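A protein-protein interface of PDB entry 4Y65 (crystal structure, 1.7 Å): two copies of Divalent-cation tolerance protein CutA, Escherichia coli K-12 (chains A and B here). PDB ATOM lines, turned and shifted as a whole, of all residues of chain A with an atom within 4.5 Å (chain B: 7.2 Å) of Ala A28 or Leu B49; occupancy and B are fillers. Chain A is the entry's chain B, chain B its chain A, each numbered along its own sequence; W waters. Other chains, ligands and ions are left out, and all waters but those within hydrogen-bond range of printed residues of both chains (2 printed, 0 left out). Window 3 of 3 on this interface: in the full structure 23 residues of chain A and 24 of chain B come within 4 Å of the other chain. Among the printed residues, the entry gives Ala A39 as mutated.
The side-chain amide oxygen (OE1) of Gln B58 sits close to the side-chain amide oxygen (OE1) of Gln A25 (3.4 Å).
The backbone carbonyl oxygen of Thr B47 is in hydrogen-bond range of the backbone NH of Leu A42 (2.6 Å).
O of Ala A40 lies within hydrogen-bond range of N of Leu B49 (2.8 Å).
The backbone carbonyl oxygen (O) of Tyr B50 sits at hydrogen-bond distance from the backbone NH (N) of Glu B57.
The side-chain carboxylate (OE1) of Glu B61 sits at hydrogen-bond distance from the side-chain hydroxyl (OG) of Ser B48, at 2.6 Å.
The backbone NH of Ser B48 is in hydrogen-bond range of the backbone carbonyl oxygen of Glu B59 (2.8 Å).
Ala A28 touches Leu B49.
Leu B49 touches Leu A32.
Tyr B51 touches Leu A32 (CE2 to O, 3.6 Å).
Leu B49 touches Ala A39 (O to CA, 3.4 Å).
CB of Ala A39 touches CB of Tyr B50 (3.9 Å).
Thr B47 touches Ala A40.
Ala A40 touches Ser B48 (O to CA, 3.4 Å).
Leu A42 touches Leu B49 (CD1 to CD1, 3.8 Å).
Printed residues of chain B within 4 Å of Ala A28: Leu B49.
Printed residues of chain A within 4 Å of Leu B49: Ala A28, Leu A32, Ala A39, Ala A40 and Leu A42.
Of the printed residues of chain B, Ala A39 touches Leu B49 and Tyr B50.
Printed residues of chain A within 4 Å of Tyr B51: Leu A32 (3.6 Å).
Of the printed residues of chain B, Leu A42 touches Thr B47 and Leu B49.
Printed residues of chain A within 4 Å of Ser B48: Ala A40 (3.4 Å).
Of the 10 printed residues of chain B, 6 touch a printed residue of chain A.
Along chain B the printed residues that touch a printed residue of chain A span positions 47 to 58.
Of the 13 printed residues of chain A, 6 touch a printed residue of chain B.
Printed residues of chain A that touch a printed residue of chain B: Gln A25, Ala A28, Leu A32, Ala A39, Ala A40 and Leu A42.
Hydrophobic or aromatic side chains of chain A that line the printed part of chain B: Ala A28, Leu A32, Ala A39 and Leu A42.
Among the printed residues, 11 pairs touch across the chains.
Among the printed residues, no Asp or Glu carboxylate lies within 4 Å of a Lys or Arg side-chain nitrogen of the other chain.
No position is printed for both chains.
Of the 11 pairs that touch across the chains among the printed residues, none has its exchanged pair printed and touching as well.
Water W2 lies within hydrogen-bond range of the side-chain hydroxyl (OH) of Tyr B51 (2.5 Å) and the backbone carbonyl oxygen (O) of Ala A29 (2.6 Å).
Water W1 bridges the side-chain amide nitrogen of Gln A25 (2.8 Å) and the side-chain hydroxyl of Thr B47 (2.9 Å).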
ATOM      1  N   ALA A  24     -15.847  23.093   9.069  1.00  0.00           N
ATOM      2  CA  ALA A  24     -14.759  22.850  10.006  1.00  0.00           C
ATOM      3  C   ALA A  24     -13.546  23.728   9.709  1.00  0.00           C
ATOM      4  O   ALA A  24     -12.962  24.317  10.613  1.00  0.00           O
ATOM      5  CB  ALA A  24     -14.365  21.384   9.975  1.00  0.00           C
ATOM      6  N   GLN A  25     -13.154  23.807   8.442  1.00  0.00           N
ATOM      7  CA  GLN A  25     -12.009  24.627   8.086  1.00  0.00           C
ATOM      8  C   GLN A  25     -12.249  26.104   8.372  1.00  0.00           C
ATOM      9  O   GLN A  25     -11.362  26.799   8.852  1.00  0.00           O
ATOM     10  CB  GLN A  25     -11.639  24.435   6.608  1.00  0.00           C
ATOM     11  CG  GLN A  25     -10.811  23.192   6.339  1.00  0.00           C
ATOM     12  CD  GLN A  25     -10.214  23.190   4.943  1.00  0.00           C
ATOM     13  OE1 GLN A  25      -9.739  24.219   4.459  1.00  0.00           O
ATOM     14  NE2 GLN A  25     -10.217  22.031   4.299  1.00  0.00           N
ATOM     15  N   ASP A  26     -13.449  26.590   8.081  1.00  0.00           N
ATOM     16  CA  ASP A  26     -13.739  27.993   8.331  1.00  0.00           C
ATOM     17  C   ASP A  26     -13.784  28.305   9.825  1.00  0.00           C
ATOM     18  O   ASP A  26     -13.319  29.353  10.249  1.00  0.00           O
ATOM     19  CB  ASP A  26     -15.045  28.400   7.646  1.00  0.00           C
ATOM     20  CG  ASP A  26     -14.957  28.303   6.125  1.00  0.00           C
ATOM     21  OD1 ASP A  26     -13.865  28.573   5.561  1.00  0.00           O
ATOM     22  OD2 ASP A  26     -15.988  27.985   5.493  1.00  0.00           O
ATOM     23  N   LEU A  27     -14.335  27.393  10.621  1.00  0.00           N
ATOM     24  CA  LEU A  27     -14.403  27.599  12.069  1.00  0.00           C
ATOM     25  C   LEU A  27     -12.987  27.650  12.626  1.00  0.00           C
ATOM     26  O   LEU A  27     -12.658  28.513  13.433  1.00  0.00           O
ATOM     27  CB  LEU A  27     -15.174  26.464  12.743  1.00  0.00           C
ATOM     28  CG  LEU A  27     -16.692  26.501  12.591  1.00  0.00           C
ATOM     29  CD1 LEU A  27     -17.288  25.204  13.099  1.00  0.00           C
ATOM     30  CD2 LEU A  27     -17.247  27.694  13.362  1.00  0.00           C
ATOM     31  N   ALA A  28     -12.155  26.708  12.193  1.00  0.00           N
ATOM     32  CA  ALA A  28     -10.770  26.649  12.638  1.00  0.00           C
ATOM     33  C   ALA A  28     -10.020  27.921  12.241  1.00  0.00           C
ATOM     34  O   ALA A  28      -9.372  28.558  13.067  1.00  0.00           O
ATOM     35  CB  ALA A  28     -10.083  25.429  12.038  1.00  0.00           C
ATOM     36  N   ALA A  29     -10.118  28.297  10.970  1.00  0.00           N
ATOM     37  CA  ALA A  29      -9.431  29.490  10.489  1.00  0.00           C
ATOM     38  C   ALA A  29      -9.822  30.710  11.324  1.00  0.00           C
ATOM     39  O   ALA A  29      -8.983  31.544  11.663  1.00  0.00           O
ATOM     40  CB  ALA A  29      -9.769  29.729   9.026  1.00  0.00           C
ATOM     41  N   LYS A  30     -11.105  30.791  11.651  1.00  0.00           N
ATOM     42  CA  LYS A  30     -11.649  31.897  12.434  1.00  0.00           C
ATOM     43  C   LYS A  30     -11.045  32.005  13.832  1.00  0.00           C
ATOM     44  O   LYS A  30     -10.483  33.038  14.198  1.00  0.00           O
ATOM     45  CB  LYS A  30     -13.163  31.734  12.552  1.00  0.00           C
ATOM     46  CG  LYS A  30     -13.862  32.794  13.384  1.00  0.00           C
ATOM     47  CD  LYS A  30     -13.885  34.132  12.677  1.00  0.00           C
ATOM     48  CE  LYS A  30     -14.741  35.130  13.438  1.00  0.00           C
ATOM     49  NZ  LYS A  30     -14.828  36.436  12.735  1.00  0.00           N
ATOM     50  N   VAL A  31     -11.165  30.942  14.619  1.00  0.00           N
ATOM     51  CA  VAL A  31     -10.637  30.980  15.979  1.00  0.00           C
ATOM     52  C   VAL A  31      -9.116  31.048  16.033  1.00  0.00           C
ATOM     53  O   VAL A  31      -8.550  31.596  16.978  1.00  0.00           O
ATOM     54  CB  VAL A  31     -11.150  29.790  16.806  1.00  0.00           C
ATOM     55  CG1 VAL A  31     -12.664  29.833  16.848  1.00  0.00           C
ATOM     56  CG2 VAL A  31     -10.668  28.469  16.208  1.00  0.00           C
ATOM     57  N   LEU A  32      -8.447  30.499  15.022  1.00  0.00           N
ATOM     58  CA  LEU A  32      -6.988  30.559  14.989  1.00  0.00           C
ATOM     59  C   LEU A  32      -6.575  32.000  14.700  1.00  0.00           C
ATOM     60  O   LEU A  32      -5.637  32.527  15.298  1.00  0.00           O
ATOM     61  CB  LEU A  32      -6.433  29.625  13.904  1.00  0.00           C
ATOM     62  CG  LEU A  32      -6.562  28.122  14.180  1.00  0.00           C
ATOM     63  CD1 LEU A  32      -6.169  27.316  12.947  1.00  0.00           C
ATOM     64  CD2 LEU A  32      -5.675  27.753  15.358  1.00  0.00           C
ATOM     65  N   ALA A  39      -3.880  25.748  17.599  1.00  0.00           N
ATOM     66  CA  ALA A  39      -3.897  24.802  16.490  1.00  0.00           C
ATOM     67  C   ALA A  39      -5.206  24.028  16.462  1.00  0.00           C
ATOM     68  O   ALA A  39      -5.890  23.907  17.479  1.00  0.00           O
ATOM     69  CB  ALA A  39      -2.717  23.832  16.614  1.00  0.00           C
ATOM     70  N   ALA A  40      -5.549  23.503  15.288  1.00  0.00           N
ATOM     71  CA  ALA A  40      -6.770  22.730  15.119  1.00  0.00           C
ATOM     72  C   ALA A  40      -6.505  21.551  14.201  1.00  0.00           C
ATOM     73  O   ALA A  40      -5.880  21.702  13.151  1.00  0.00           O
ATOM     74  CB  ALA A  40      -7.873  23.605  14.526  1.00  0.00           C
ATOM     75  N   LEU A  42      -8.429  18.544  12.127  1.00  0.00           N
ATOM     76  CA  LEU A  42      -9.736  18.179  11.603  1.00  0.00           C
ATOM     77  C   LEU A  42      -9.709  16.765  11.045  1.00  0.00           C
ATOM     78  O   LEU A  42      -8.811  16.408  10.289  1.00  0.00           O
ATOM     79  CB  LEU A  42     -10.138  19.137  10.477  1.00  0.00           C
ATOM     80  CG  LEU A  42      -9.915  20.633  10.706  1.00  0.00           C
ATOM     81  CD1 LEU A  42     -10.365  21.406   9.462  1.00  0.00           C
ATOM     82  CD2 LEU A  42     -10.676  21.091  11.935  1.00  0.00           C
ATOM     83  N   MET A  64     -13.253  17.645  15.370  1.00  0.00           N
ATOM     84  CA  MET A  64     -12.243  18.685  15.510  1.00  0.00           C
ATOM     85  C   MET A  64     -11.569  18.545  16.867  1.00  0.00           C
ATOM     86  O   MET A  64     -12.215  18.195  17.851  1.00  0.00           O
ATOM     87  CB  MET A  64     -12.876  20.079  15.417  1.00  0.00           C
ATOM     88  CG  MET A  64     -13.543  20.392  14.095  1.00  0.00           C
ATOM     89  SD  MET A  64     -14.349  22.006  14.153  1.00  0.00           S
ATOM     90  CE  MET A  64     -12.961  23.075  13.930  1.00  0.00           C
ATOM     91  N   THR B  47      -6.401  16.869   8.926  1.00  0.00           N
ATOM     92  CA  THR B  47      -5.914  18.162   8.461  1.00  0.00           C
ATOM     93  C   THR B  47      -5.535  18.983   9.691  1.00  0.00           C
ATOM     94  O   THR B  47      -6.308  19.065  10.644  1.00  0.00           O
ATOM     95  CB  THR B  47      -6.996  18.943   7.686  1.00  0.00           C
ATOM     96  OG1 THR B  47      -7.348  18.230   6.495  1.00  0.00           O
ATOM     97  CG2 THR B  47      -6.481  20.332   7.309  1.00  0.00           C
ATOM     98  N   SER B  48      -4.349  19.579   9.665  1.00  0.00           N
ATOM     99  CA  SER B  48      -3.878  20.395  10.776  1.00  0.00           C
ATOM    100  C   SER B  48      -3.704  21.842  10.342  1.00  0.00           C
ATOM    101  O   SER B  48      -3.064  22.118   9.333  1.00  0.00           O
ATOM    102  CB  SER B  48      -2.543  19.864  11.297  1.00  0.00           C
ATOM    103  OG  SER B  48      -2.689  18.557  11.820  1.00  0.00           O
ATOM    104  N   LEU B  49      -4.296  22.763  11.097  1.00  0.00           N
ATOM    105  CA  LEU B  49      -4.178  24.183  10.791  1.00  0.00           C
ATOM    106  C   LEU B  49      -3.548  24.878  11.989  1.00  0.00           C
ATOM    107  O   LEU B  49      -3.884  24.575  13.135  1.00  0.00           O
ATOM    108  CB  LEU B  49      -5.551  24.809  10.513  1.00  0.00           C
ATOM    109  CG  LEU B  49      -6.343  24.332   9.296  1.00  0.00           C
ATOM    110  CD1 LEU B  49      -6.899  22.946   9.552  1.00  0.00           C
ATOM    111  CD2 LEU B  49      -7.480  25.298   9.029  1.00  0.00           C
ATOM    112  N   TYR B  50      -2.628  25.795  11.711  1.00  0.00           N
ATOM    113  CA  TYR B  50      -1.942  26.560  12.744  1.00  0.00           C
ATOM    114  C   TYR B  50      -1.097  27.623  12.066  1.00  0.00           C
ATOM    115  O   TYR B  50      -0.757  27.496  10.893  1.00  0.00           O
ATOM    116  CB  TYR B  50      -1.026  25.654  13.575  1.00  0.00           C
ATOM    117  CG  TYR B  50       0.006  24.919  12.751  1.00  0.00           C
ATOM    118  CD1 TYR B  50      -0.321  23.739  12.078  1.00  0.00           C
ATOM    119  CD2 TYR B  50       1.306  25.410  12.625  1.00  0.00           C
ATOM    120  CE1 TYR B  50       0.623  23.066  11.300  1.00  0.00           C
ATOM    121  CE2 TYR B  50       2.257  24.745  11.850  1.00  0.00           C
ATOM    122  CZ  TYR B  50       1.909  23.575  11.193  1.00  0.00           C
ATOM    123  OH  TYR B  50       2.851  22.913  10.440  1.00  0.00           O
ATOM    124  N   TYR B  51      -0.764  28.672  12.809  1.00  0.00           N
ATOM    125  CA  TYR B  51       0.068  29.742  12.287  1.00  0.00           C
ATOM    126  C   TYR B  51       1.519  29.449  12.645  1.00  0.00           C
ATOM    127  O   TYR B  51       1.813  28.947  13.731  1.00  0.00           O
ATOM    128  CB  TYR B  51      -0.352  31.081  12.894  1.00  0.00           C
ATOM    129  CG  TYR B  51      -1.596  31.661  12.265  1.00  0.00           C
ATOM    130  CD1 TYR B  51      -1.509  32.486  11.145  1.00  0.00           C
ATOM    131  CD2 TYR B  51      -2.860  31.358  12.765  1.00  0.00           C
ATOM    132  CE1 TYR B  51      -2.654  33.000  10.538  1.00  0.00           C
ATOM    133  CE2 TYR B  51      -4.013  31.865  12.164  1.00  0.00           C
ATOM    134  CZ  TYR B  51      -3.898  32.685  11.053  1.00  0.00           C
ATOM    135  OH  TYR B  51      -5.028  33.191  10.456  1.00  0.00           O
ATOM    136  N   LEU B  56      -0.569  31.204   8.016  1.00  0.00           N
ATOM    137  CA  LEU B  56      -1.422  30.043   8.240  1.00  0.00           C
ATOM    138  C   LEU B  56      -0.944  28.828   7.450  1.00  0.00           C
ATOM    139  O   LEU B  56      -0.844  28.869   6.223  1.00  0.00           O
ATOM    140  CB  LEU B  56      -2.868  30.366   7.850  1.00  0.00           C
ATOM    141  CG  LEU B  56      -3.899  29.256   8.082  1.00  0.00           C
ATOM    142  CD1 LEU B  56      -3.972  28.932   9.569  1.00  0.00           C
ATOM    143  CD2 LEU B  56      -5.259  29.698   7.565  1.00  0.00           C
ATOM    144  N   GLU B  57      -0.652  27.749   8.167  1.00  0.00           N
ATOM    145  CA  GLU B  57      -0.198  26.507   7.551  1.00  0.00           C
ATOM    146  C   GLU B  57      -1.335  25.489   7.564  1.00  0.00           C
ATOM    147  O   GLU B  57      -2.167  25.475   8.474  1.00  0.00           O
ATOM    148  CB  GLU B  57       0.998  25.934   8.318  1.00  0.00           C
ATOM    149  CG  GLU B  57       2.250  26.809   8.323  1.00  0.00           C
ATOM    150  CD  GLU B  57       2.877  26.954   6.952  1.00  0.00           C
ATOM    151  OE1 GLU B  57       2.984  25.938   6.233  1.00  0.00           O
ATOM    152  OE2 GLU B  57       3.279  28.081   6.594  1.00  0.00           O
ATOM    153  N   GLN B  58      -1.371  24.639   6.547  1.00  0.00           N
ATOM    154  CA  GLN B  58      -2.390  23.606   6.455  1.00  0.00           C
ATOM    155  C   GLN B  58      -1.683  22.331   6.030  1.00  0.00           C
ATOM    156  O   GLN B  58      -1.279  22.198   4.875  1.00  0.00           O
ATOM    157  CB  GLN B  58      -3.457  23.990   5.424  1.00  0.00           C
ATOM    158  CG  GLN B  58      -4.566  22.957   5.268  1.00  0.00           C
ATOM    159  CD  GLN B  58      -5.755  23.474   4.475  1.00  0.00           C
ATOM    160  OE1 GLN B  58      -6.419  24.432   4.879  1.00  0.00           O
ATOM    161  NE2 GLN B  58      -6.031  22.840   3.341  1.00  0.00           N
ATOM    162  N   GLU B  59      -1.516  21.404   6.967  1.00  0.00           N
ATOM    163  CA  GLU B  59      -0.839  20.146   6.674  1.00  0.00           C
ATOM    164  C   GLU B  59      -1.794  18.964   6.728  1.00  0.00           C
ATOM    165  O   GLU B  59      -2.787  18.982   7.448  1.00  0.00           O
ATOM    166  CB  GLU B  59       0.308  19.918   7.667  1.00  0.00           C
ATOM    167  CG  GLU B  59       1.445  20.924   7.549  1.00  0.00           C
ATOM    168  CD  GLU B  59       2.086  20.922   6.171  1.00  0.00           C
ATOM    169  OE1 GLU B  59       2.498  19.835   5.707  1.00  0.00           O
ATOM    170  OE2 GLU B  59       2.181  22.006   5.552  1.00  0.00           O
ATOM    171  N   GLU B  61      -1.946  15.329   7.858  1.00  0.00           N
ATOM    172  CA  GLU B  61      -1.180  14.422   8.691  1.00  0.00           C
ATOM    173  C   GLU B  61      -1.954  13.235   9.226  1.00  0.00           C
ATOM    174  O   GLU B  61      -3.104  12.991   8.859  1.00  0.00           O
ATOM    175  CB  GLU B  61      -0.613  15.209   9.874  1.00  0.00           C
ATOM    176  CG  GLU B  61      -0.164  16.617   9.505  1.00  0.00           C
ATOM    177  CD  GLU B  61       0.407  17.382  10.682  1.00  0.00           C
ATOM    178  OE1 GLU B  61      -0.308  17.551  11.695  1.00  0.00           O
ATOM    179  OE2 GLU B  61       1.571  17.818  10.588  1.00  0.00           O
HETATM  180  O   HOH W   1      -9.644  19.557   5.355  1.00  0.00           O
HETATM  181  O   HOH W   2      -6.958  31.597  10.041  1.00  0.00           O
